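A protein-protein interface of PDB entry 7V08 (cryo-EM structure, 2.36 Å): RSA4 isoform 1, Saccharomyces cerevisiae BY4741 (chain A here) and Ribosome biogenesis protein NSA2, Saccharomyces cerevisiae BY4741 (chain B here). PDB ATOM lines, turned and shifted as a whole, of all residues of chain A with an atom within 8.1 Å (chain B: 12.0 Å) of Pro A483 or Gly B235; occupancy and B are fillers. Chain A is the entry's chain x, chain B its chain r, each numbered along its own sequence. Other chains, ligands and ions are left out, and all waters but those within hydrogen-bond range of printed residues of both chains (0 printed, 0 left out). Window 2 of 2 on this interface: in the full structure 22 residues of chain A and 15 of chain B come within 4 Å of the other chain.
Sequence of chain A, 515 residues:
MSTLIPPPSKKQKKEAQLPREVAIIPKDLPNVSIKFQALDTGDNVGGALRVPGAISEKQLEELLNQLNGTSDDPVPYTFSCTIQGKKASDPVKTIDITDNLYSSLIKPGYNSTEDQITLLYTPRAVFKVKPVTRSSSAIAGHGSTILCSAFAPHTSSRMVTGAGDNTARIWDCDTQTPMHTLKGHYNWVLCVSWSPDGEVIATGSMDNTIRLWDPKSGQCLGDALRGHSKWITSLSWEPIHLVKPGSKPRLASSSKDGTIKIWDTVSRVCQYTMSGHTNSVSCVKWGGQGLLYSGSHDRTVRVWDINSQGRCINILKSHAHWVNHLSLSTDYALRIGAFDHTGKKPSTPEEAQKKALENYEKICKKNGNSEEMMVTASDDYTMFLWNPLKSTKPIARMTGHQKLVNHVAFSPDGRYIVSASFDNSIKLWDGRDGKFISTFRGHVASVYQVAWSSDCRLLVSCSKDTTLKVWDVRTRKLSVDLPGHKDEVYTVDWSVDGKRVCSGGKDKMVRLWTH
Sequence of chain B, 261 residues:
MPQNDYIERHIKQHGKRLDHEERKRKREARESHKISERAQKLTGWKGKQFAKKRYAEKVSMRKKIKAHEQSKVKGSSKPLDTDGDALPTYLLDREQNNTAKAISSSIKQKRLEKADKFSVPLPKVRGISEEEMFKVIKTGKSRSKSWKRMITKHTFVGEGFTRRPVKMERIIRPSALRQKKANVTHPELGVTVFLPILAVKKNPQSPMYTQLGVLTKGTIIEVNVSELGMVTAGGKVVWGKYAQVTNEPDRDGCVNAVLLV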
ATOM      1  N   THR A 133     -28.067  38.211  10.191  1.00  0.00           N
ATOM      2  CA  THR A 133     -27.238  37.115   9.712  1.00  0.00           C
ATOM      3  C   THR A 133     -26.151  36.688  10.683  1.00  0.00           C
ATOM      4  O   THR A 133     -25.555  35.625  10.485  1.00  0.00           O
ATOM      5  CB  THR A 133     -26.591  37.497   8.378  1.00  0.00           C
ATOM      6  OG1 THR A 133     -25.906  38.746   8.523  1.00  0.00           O
ATOM      7  CG2 THR A 133     -27.642  37.615   7.284  1.00  0.00           C
ATOM      8  N   ARG A 134     -25.877  37.467  11.720  1.00  0.00           N
ATOM      9  CA  ARG A 134     -24.737  37.178  12.575  1.00  0.00           C
ATOM     10  C   ARG A 134     -25.003  37.750  13.953  1.00  0.00           C
ATOM     11  O   ARG A 134     -25.752  38.713  14.108  1.00  0.00           O
ATOM     12  CB  ARG A 134     -23.442  37.758  11.995  1.00  0.00           C
ATOM     13  CG  ARG A 134     -23.580  39.170  11.450  1.00  0.00           C
ATOM     14  CD  ARG A 134     -22.437  39.530  10.512  1.00  0.00           C
ATOM     15  NE  ARG A 134     -22.476  40.934  10.129  1.00  0.00           N
ATOM     16  CZ  ARG A 134     -21.985  41.921  10.866  1.00  0.00           C
ATOM     17  NH1 ARG A 134     -21.393  41.689  12.024  1.00  0.00           N
ATOM     18  NH2 ARG A 134     -22.089  43.171  10.429  1.00  0.00           N
ATOM     19  N   SER A 135     -24.366  37.150  14.951  1.00  0.00           N
ATOM     20  CA  SER A 135     -24.486  37.610  16.324  1.00  0.00           C
ATOM     21  C   SER A 135     -23.573  38.811  16.507  1.00  0.00           C
ATOM     22  O   SER A 135     -22.345  38.670  16.475  1.00  0.00           O
ATOM     23  CB  SER A 135     -24.122  36.500  17.310  1.00  0.00           C
ATOM     24  OG  SER A 135     -24.410  36.888  18.646  1.00  0.00           O
ATOM     25  N   GLY A 442     -38.098  23.228  10.523  1.00  0.00           N
ATOM     26  CA  GLY A 442     -36.668  23.388  10.671  1.00  0.00           C
ATOM     27  C   GLY A 442     -36.194  23.445  12.106  1.00  0.00           C
ATOM     28  O   GLY A 442     -35.062  23.057  12.396  1.00  0.00           O
ATOM     29  N   VAL A 444     -36.055  21.664  15.507  1.00  0.00           N
ATOM     30  CA  VAL A 444     -36.166  20.272  15.917  1.00  0.00           C
ATOM     31  C   VAL A 444     -36.675  20.123  17.340  1.00  0.00           C
ATOM     32  O   VAL A 444     -36.749  19.000  17.852  1.00  0.00           O
ATOM     33  CB  VAL A 444     -34.819  19.539  15.745  1.00  0.00           C
ATOM     34  CG1 VAL A 444     -34.513  19.369  14.273  1.00  0.00           C
ATOM     35  CG2 VAL A 444     -33.706  20.296  16.441  1.00  0.00           C
ATOM     36  N   ASP A 465     -34.427  24.292  20.950  1.00  0.00           N
ATOM     37  CA  ASP A 465     -33.230  23.665  20.400  1.00  0.00           C
ATOM     38  C   ASP A 465     -32.028  24.603  20.379  1.00  0.00           C
ATOM     39  O   ASP A 465     -31.089  24.383  19.605  1.00  0.00           O
ATOM     40  CB  ASP A 465     -33.507  23.103  19.000  1.00  0.00           C
ATOM     41  CG  ASP A 465     -33.850  24.179  17.950  1.00  0.00           C
ATOM     42  OD1 ASP A 465     -33.647  25.389  18.172  1.00  0.00           O
ATOM     43  OD2 ASP A 465     -34.342  23.799  16.873  1.00  0.00           O
ATOM     44  N   THR A 466     -32.050  25.648  21.210  1.00  0.00           N
ATOM     45  CA  THR A 466     -30.977  26.629  21.383  1.00  0.00           C
ATOM     46  C   THR A 466     -30.645  27.384  20.099  1.00  0.00           C
ATOM     47  O   THR A 466     -29.512  27.849  19.936  1.00  0.00           O
ATOM     48  CB  THR A 466     -29.694  25.992  21.951  1.00  0.00           C
ATOM     49  OG1 THR A 466     -28.963  25.344  20.904  1.00  0.00           O
ATOM     50  CG2 THR A 466     -30.010  24.979  23.049  1.00  0.00           C
ATOM     51  N   THR A 467     -31.596  27.544  19.176  1.00  0.00           N
ATOM     52  CA  THR A 467     -31.349  28.273  17.937  1.00  0.00           C
ATOM     53  C   THR A 467     -32.441  29.303  17.686  1.00  0.00           C
ATOM     54  O   THR A 467     -33.587  29.173  18.149  1.00  0.00           O
ATOM     55  CB  THR A 467     -31.261  27.364  16.676  1.00  0.00           C
ATOM     56  OG1 THR A 467     -32.574  26.968  16.260  1.00  0.00           O
ATOM     57  CG2 THR A 467     -30.405  26.135  16.912  1.00  0.00           C
ATOM     58  N   LEU A 468     -32.053  30.335  16.940  1.00  0.00           N
ATOM     59  CA  LEU A 468     -32.973  31.262  16.310  1.00  0.00           C
ATOM     60  C   LEU A 468     -33.068  30.923  14.830  1.00  0.00           C
ATOM     61  O   LEU A 468     -32.142  30.354  14.246  1.00  0.00           O
ATOM     62  CB  LEU A 468     -32.511  32.713  16.470  1.00  0.00           C
ATOM     63  CG  LEU A 468     -32.923  33.553  17.674  1.00  0.00           C
ATOM     64  CD1 LEU A 468     -32.516  32.906  18.975  1.00  0.00           C
ATOM     65  CD2 LEU A 468     -32.284  34.921  17.548  1.00  0.00           C
ATOM     66  N   LYS A 469     -34.191  31.276  14.220  1.00  0.00           N
ATOM     67  CA  LYS A 469     -34.361  31.049  12.793  1.00  0.00           C
ATOM     68  C   LYS A 469     -35.085  32.227  12.167  1.00  0.00           C
ATOM     69  O   LYS A 469     -36.088  32.697  12.708  1.00  0.00           O
ATOM     70  CB  LYS A 469     -35.119  29.745  12.530  1.00  0.00           C
ATOM     71  CG  LYS A 469     -34.240  28.513  12.625  1.00  0.00           C
ATOM     72  CD  LYS A 469     -34.946  27.251  12.208  1.00  0.00           C
ATOM     73  CE  LYS A 469     -33.935  26.144  11.970  1.00  0.00           C
ATOM     74  NZ  LYS A 469     -32.952  26.075  13.075  1.00  0.00           N
ATOM     75  N   VAL A 480     -32.341  32.053   7.129  1.00  0.00           N
ATOM     76  CA  VAL A 480     -31.043  31.849   7.770  1.00  0.00           C
ATOM     77  C   VAL A 480     -31.243  31.284   9.172  1.00  0.00           C
ATOM     78  O   VAL A 480     -32.066  31.776   9.948  1.00  0.00           O
ATOM     79  CB  VAL A 480     -30.212  33.155   7.777  1.00  0.00           C
ATOM     80  CG1 VAL A 480     -31.067  34.342   8.133  1.00  0.00           C
ATOM     81  CG2 VAL A 480     -29.013  33.052   8.711  1.00  0.00           C
ATOM     82  N   ASP A 481     -30.485  30.239   9.489  1.00  0.00           N
ATOM     83  CA  ASP A 481     -30.486  29.622  10.810  1.00  0.00           C
ATOM     84  C   ASP A 481     -29.342  30.200  11.631  1.00  0.00           C
ATOM     85  O   ASP A 481     -28.204  30.260  11.157  1.00  0.00           O
ATOM     86  CB  ASP A 481     -30.357  28.103  10.692  1.00  0.00           C
ATOM     87  CG  ASP A 481     -30.171  27.419  12.031  1.00  0.00           C
ATOM     88  OD1 ASP A 481     -31.065  27.543  12.893  1.00  0.00           O
ATOM     89  OD2 ASP A 481     -29.134  26.746  12.213  1.00  0.00           O
ATOM     90  N   LEU A 482     -29.645  30.640  12.850  1.00  0.00           N
ATOM     91  CA  LEU A 482     -28.679  31.324  13.706  1.00  0.00           C
ATOM     92  C   LEU A 482     -28.430  30.513  14.970  1.00  0.00           C
ATOM     93  O   LEU A 482     -29.266  30.518  15.894  1.00  0.00           O
ATOM     94  CB  LEU A 482     -29.177  32.725  14.057  1.00  0.00           C
ATOM     95  CG  LEU A 482     -29.598  33.638  12.901  1.00  0.00           C
ATOM     96  CD1 LEU A 482     -30.463  34.778  13.413  1.00  0.00           C
ATOM     97  CD2 LEU A 482     -28.392  34.188  12.165  1.00  0.00           C
ATOM     98  N   PRO A 483     -27.323  29.769  15.044  1.00  0.00           N
ATOM     99  CA  PRO A 483     -26.920  29.173  16.323  1.00  0.00           C
ATOM    100  C   PRO A 483     -26.012  30.097  17.113  1.00  0.00           C
ATOM    101  O   PRO A 483     -25.616  31.157  16.622  1.00  0.00           O
ATOM    102  CB  PRO A 483     -26.191  27.898  15.891  1.00  0.00           C
ATOM    103  CG  PRO A 483     -25.610  28.250  14.582  1.00  0.00           C
ATOM    104  CD  PRO A 483     -26.550  29.218  13.919  1.00  0.00           C
ATOM    105  N   GLY A 484     -25.656  29.696  18.326  1.00  0.00           N
ATOM    106  CA  GLY A 484     -24.796  30.508  19.161  1.00  0.00           C
ATOM    107  C   GLY A 484     -25.173  30.489  20.625  1.00  0.00           C
ATOM    108  O   GLY A 484     -24.296  30.550  21.490  1.00  0.00           O
ATOM    109  N   HIS A 485     -26.463  30.383  20.925  1.00  0.00           N
ATOM    110  CA  HIS A 485     -26.877  30.196  22.307  1.00  0.00           C
ATOM    111  C   HIS A 485     -26.449  28.820  22.803  1.00  0.00           C
ATOM    112  O   HIS A 485     -26.543  27.826  22.081  1.00  0.00           O
ATOM    113  CB  HIS A 485     -28.389  30.343  22.446  1.00  0.00           C
ATOM    114  CG  HIS A 485     -28.861  31.759  22.515  1.00  0.00           C
ATOM    115  ND1 HIS A 485     -28.886  32.475  23.691  1.00  0.00           N
ATOM    116  CD2 HIS A 485     -29.345  32.586  21.560  1.00  0.00           C
ATOM    117  CE1 HIS A 485     -29.364  33.683  23.459  1.00  0.00           C
ATOM    118  NE2 HIS A 485     -29.643  33.779  22.172  1.00  0.00           N
ATOM    119  N   LYS A 486     -25.969  28.771  24.043  1.00  0.00           N
ATOM    120  CA  LYS A 486     -25.553  27.513  24.652  1.00  0.00           C
ATOM    121  C   LYS A 486     -26.712  26.705  25.223  1.00  0.00           C
ATOM    122  O   LYS A 486     -26.571  25.489  25.386  1.00  0.00           O
ATOM    123  CB  LYS A 486     -24.543  27.779  25.767  1.00  0.00           C
ATOM    124  CG  LYS A 486     -23.341  28.583  25.344  1.00  0.00           C
ATOM    125  CD  LYS A 486     -22.435  27.780  24.440  1.00  0.00           C
ATOM    126  CE  LYS A 486     -21.198  28.576  24.072  1.00  0.00           C
ATOM    127  NZ  LYS A 486     -20.520  29.124  25.283  1.00  0.00           N
ATOM    128  N   ARG A 511     -28.198  38.138  23.579  1.00  0.00           N
ATOM    129  CA  ARG A 511     -27.579  38.056  22.265  1.00  0.00           C
ATOM    130  C   ARG A 511     -28.200  39.099  21.348  1.00  0.00           C
ATOM    131  O   ARG A 511     -29.422  39.116  21.159  1.00  0.00           O
ATOM    132  CB  ARG A 511     -27.736  36.657  21.675  1.00  0.00           C
ATOM    133  CG  ARG A 511     -26.897  35.611  22.373  1.00  0.00           C
ATOM    134  CD  ARG A 511     -25.445  35.798  22.085  1.00  0.00           C
ATOM    135  NE  ARG A 511     -25.028  35.156  20.848  1.00  0.00           N
ATOM    136  CZ  ARG A 511     -24.039  34.277  20.760  1.00  0.00           C
ATOM    137  NH1 ARG A 511     -23.350  33.904  21.824  1.00  0.00           N
ATOM    138  NH2 ARG A 511     -23.724  33.776  19.572  1.00  0.00           N
ATOM    139  N   TRP A 513     -28.190  40.484  17.446  1.00  0.00           N
ATOM    140  CA  TRP A 513     -27.970  39.970  16.101  1.00  0.00           C
ATOM    141  C   TRP A 513     -28.267  41.059  15.080  1.00  0.00           C
ATOM    142  O   TRP A 513     -29.251  41.794  15.216  1.00  0.00           O
ATOM    143  CB  TRP A 513     -28.871  38.763  15.801  1.00  0.00           C
ATOM    144  CG  TRP A 513     -28.973  37.728  16.877  1.00  0.00           C
ATOM    145  CD1 TRP A 513     -29.731  37.791  18.009  1.00  0.00           C
ATOM    146  CD2 TRP A 513     -28.332  36.449  16.897  1.00  0.00           C
ATOM    147  NE1 TRP A 513     -29.579  36.645  18.744  1.00  0.00           N
ATOM    148  CE2 TRP A 513     -28.724  35.804  18.082  1.00  0.00           C
ATOM    149  CE3 TRP A 513     -27.455  35.791  16.033  1.00  0.00           C
ATOM    150  CZ2 TRP A 513     -28.272  34.532  18.423  1.00  0.00           C
ATOM    151  CZ3 TRP A 513     -27.003  34.533  16.376  1.00  0.00           C
ATOM    152  CH2 TRP A 513     -27.416  33.915  17.558  1.00  0.00           C
ATOM    153  N   GLY B 229     -33.833  16.575  19.716  1.00  0.00           N
ATOM    154  CA  GLY B 229     -33.599  17.933  19.261  1.00  0.00           C
ATOM    155  C   GLY B 229     -32.258  18.551  19.608  1.00  0.00           C
ATOM    156  O   GLY B 229     -32.212  19.682  20.096  1.00  0.00           O
ATOM    157  N   MET B 230     -31.164  17.832  19.372  1.00  0.00           N
ATOM    158  CA  MET B 230     -29.829  18.318  19.698  1.00  0.00           C
ATOM    159  C   MET B 230     -29.211  19.035  18.503  1.00  0.00           C
ATOM    160  O   MET B 230     -29.351  18.588  17.361  1.00  0.00           O
ATOM    161  CB  MET B 230     -28.931  17.163  20.130  1.00  0.00           C
ATOM    162  CG  MET B 230     -29.324  16.516  21.436  1.00  0.00           C
ATOM    163  SD  MET B 230     -28.563  14.893  21.597  1.00  0.00           S
ATOM    164  CE  MET B 230     -28.856  14.550  23.322  1.00  0.00           C
ATOM    165  N   VAL B 231     -28.537  20.153  18.770  1.00  0.00           N
ATOM    166  CA  VAL B 231     -27.877  20.947  17.741  1.00  0.00           C
ATOM    167  C   VAL B 231     -26.432  21.184  18.161  1.00  0.00           C
ATOM    168  O   VAL B 231     -26.160  21.496  19.324  1.00  0.00           O
ATOM    169  CB  VAL B 231     -28.603  22.290  17.490  1.00  0.00           C
ATOM    170  CG1 VAL B 231     -27.925  23.070  16.372  1.00  0.00           C
ATOM    171  CG2 VAL B 231     -30.056  22.060  17.128  1.00  0.00           C
ATOM    172  N   THR B 232     -25.507  21.033  17.216  1.00  0.00           N
ATOM    173  CA  THR B 232     -24.098  21.307  17.473  1.00  0.00           C
ATOM    174  C   THR B 232     -23.867  22.815  17.549  1.00  0.00           C
ATOM    175  O   THR B 232     -24.771  23.623  17.325  1.00  0.00           O
ATOM    176  CB  THR B 232     -23.213  20.681  16.396  1.00  0.00           C
ATOM    177  OG1 THR B 232     -23.247  21.498  15.221  1.00  0.00           O
ATOM    178  CG2 THR B 232     -23.688  19.298  16.044  1.00  0.00           C
ATOM    179  N   ALA B 233     -22.632  23.212  17.861  1.00  0.00           N
ATOM    180  CA  ALA B 233     -22.302  24.633  17.924  1.00  0.00           C
ATOM    181  C   ALA B 233     -22.308  25.276  16.545  1.00  0.00           C
ATOM    182  O   ALA B 233     -22.453  26.497  16.435  1.00  0.00           O
ATOM    183  CB  ALA B 233     -20.946  24.827  18.594  1.00  0.00           C
ATOM    184  N   GLY B 234     -22.154  24.482  15.491  1.00  0.00           N
ATOM    185  CA  GLY B 234     -22.193  24.957  14.127  1.00  0.00           C
ATOM    186  C   GLY B 234     -23.558  24.964  13.477  1.00  0.00           C
ATOM    187  O   GLY B 234     -23.658  25.282  12.288  1.00  0.00           O
ATOM    188  N   GLY B 235     -24.612  24.622  14.209  1.00  0.00           N
ATOM    189  CA  GLY B 235     -25.949  24.591  13.657  1.00  0.00           C
ATOM    190  C   GLY B 235     -26.374  23.283  13.032  1.00  0.00           C
ATOM    191  O   GLY B 235     -27.495  23.201  12.520  1.00  0.00           O
ATOM    192  N   LYS B 236     -25.522  22.263  13.056  1.00  0.00           N
ATOM    193  CA  LYS B 236     -25.884  20.946  12.555  1.00  0.00           C
ATOM    194  C   LYS B 236     -26.807  20.240  13.539  1.00  0.00           C
ATOM    195  O   LYS B 236     -26.689  20.411  14.753  1.00  0.00           O
ATOM    196  CB  LYS B 236     -24.632  20.099  12.323  1.00  0.00           C
ATOM    197  CG  LYS B 236     -24.083  20.104  10.909  1.00  0.00           C
ATOM    198  CD  LYS B 236     -23.421  21.413  10.555  1.00  0.00           C
ATOM    199  CE  LYS B 236     -22.611  21.280   9.275  1.00  0.00           C
ATOM    200  NZ  LYS B 236     -21.967  22.563   8.906  1.00  0.00           N
ATOM    201  N   VAL B 237     -27.725  19.440  13.010  1.00  0.00           N
ATOM    202  CA  VAL B 237     -28.621  18.647  13.844  1.00  0.00           C
ATOM    203  C   VAL B 237     -27.961  17.307  14.142  1.00  0.00           C
ATOM    204  O   VAL B 237     -27.572  16.578  13.228  1.00  0.00           O
ATOM    205  CB  VAL B 237     -29.987  18.457  13.167  1.00  0.00           C
ATOM    206  CG1 VAL B 237     -30.790  17.352  13.844  1.00  0.00           C
ATOM    207  CG2 VAL B 237     -30.767  19.758  13.174  1.00  0.00           C
ATOM    208  N   VAL B 238     -27.840  16.979  15.420  1.00  0.00           N
ATOM    209  CA  VAL B 238     -27.358  15.665  15.825  1.00  0.00           C
ATOM    210  C   VAL B 238     -28.493  14.666  15.666  1.00  0.00           C
ATOM    211  O   VAL B 238     -29.617  14.913  16.117  1.00  0.00           O
ATOM    212  CB  VAL B 238     -26.848  15.692  17.275  1.00  0.00           C
ATOM    213  CG1 VAL B 238     -26.111  14.407  17.610  1.00  0.00           C
ATOM    214  CG2 VAL B 238     -25.973  16.907  17.515  1.00  0.00           C
ATOM    215  N   TRP B 239     -28.217  13.539  15.011  1.00  0.00           N
ATOM    216  CA  TRP B 239     -29.199  12.466  14.961  1.00  0.00           C
ATOM    217  C   TRP B 239     -28.587  11.104  15.261  1.00  0.00           C
ATOM    218  O   TRP B 239     -29.283  10.090  15.155  1.00  0.00           O
ATOM    219  CB  TRP B 239     -29.945  12.454  13.617  1.00  0.00           C
ATOM    220  CG  TRP B 239     -29.190  11.986  12.426  1.00  0.00           C
ATOM    221  CD1 TRP B 239     -28.319  12.711  11.672  1.00  0.00           C
ATOM    222  CD2 TRP B 239     -29.267  10.694  11.816  1.00  0.00           C
ATOM    223  NE1 TRP B 239     -27.840  11.951  10.648  1.00  0.00           N
ATOM    224  CE2 TRP B 239     -28.408  10.708  10.708  1.00  0.00           C
ATOM    225  CE3 TRP B 239     -29.978   9.527  12.103  1.00  0.00           C
ATOM    226  CZ2 TRP B 239     -28.233   9.601   9.888  1.00  0.00           C
ATOM    227  CZ3 TRP B 239     -29.803   8.431  11.288  1.00  0.00           C
ATOM    228  CH2 TRP B 239     -28.939   8.475  10.194  1.00  0.00           C
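The backbone NH of Val A444 lies within hydrogen-bond range of the side-chain carboxylate of Asp A465, at 3.1 Å. The side-chain amino group (NZ) of Lys A469 is in salt-bridge range of the side-chain carboxylate (OD2) of Asp A481 (3.97 Å). The side-chain carboxylate (OD1) of Asp A465 is in hydrogen-bond range of the side-chain hydroxyl (OG1) of Thr A467 (2.7 Å). The side-chain hydroxyl (OG1) of Thr A467 is in hydrogen-bond range of the side-chain amino group (NZ) of Lys A469 (3.3 Å).
Among the printed residues, merely in contact across the chains: Val A444 with Gly B229 (3.6 Å), Val A444 with Val B237 (3.9 Å), Asp A465 with Gly B229 (3.8 Å), Asp A465 with Val B231 (3.5 Å), Thr A467 with Val B231 (3.98 Å), Asp A481 with Gly B235 (3.9 Å) and Pro A483 with Gly B235 (3.8 Å).
Pro A483 touches just one residue of chain B: Gly B235. Of chain A, only Asp A481 and Pro A483 come within 4 Å of Gly B235. No residue of chain B comes within 4 Å of Leu A468. No residue of chain A comes within 4 Å of Gly B234. Of the printed residues of chain A, Val B237 touches Val A444. Of the printed residues of chain A, Val B231 touches Asp A465 and Thr A467. Printed residues of chain A within 4 Å of Gly B229: Val A444 and Asp A465. Of the printed residues of chain B, Asp A465 touches Gly B229 (3.8 Å) and Val B231 (3.5 Å). Of the printed residues of chain B, Val A444 touches Gly B229 and Val B237. Lys A486 touches none of the printed residues of chain B. Lys B236 touches none of the printed residues of chain A. The nearest printed residue of chain B that does not touch Pro A483 is Gly B234 (4.03 Å). The nearest printed residue of chain A that does not touch Val B231 is Val A444 (4.1 Å).
Of the 11 printed residues of chain B, 4 touch a printed residue of chain A. Hydrophobic or aromatic side chains of chain A within 4 Å of the printed part of chain B: Val A444 and Pro A483. Among the printed residues, 7 pairs touch across the chains.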
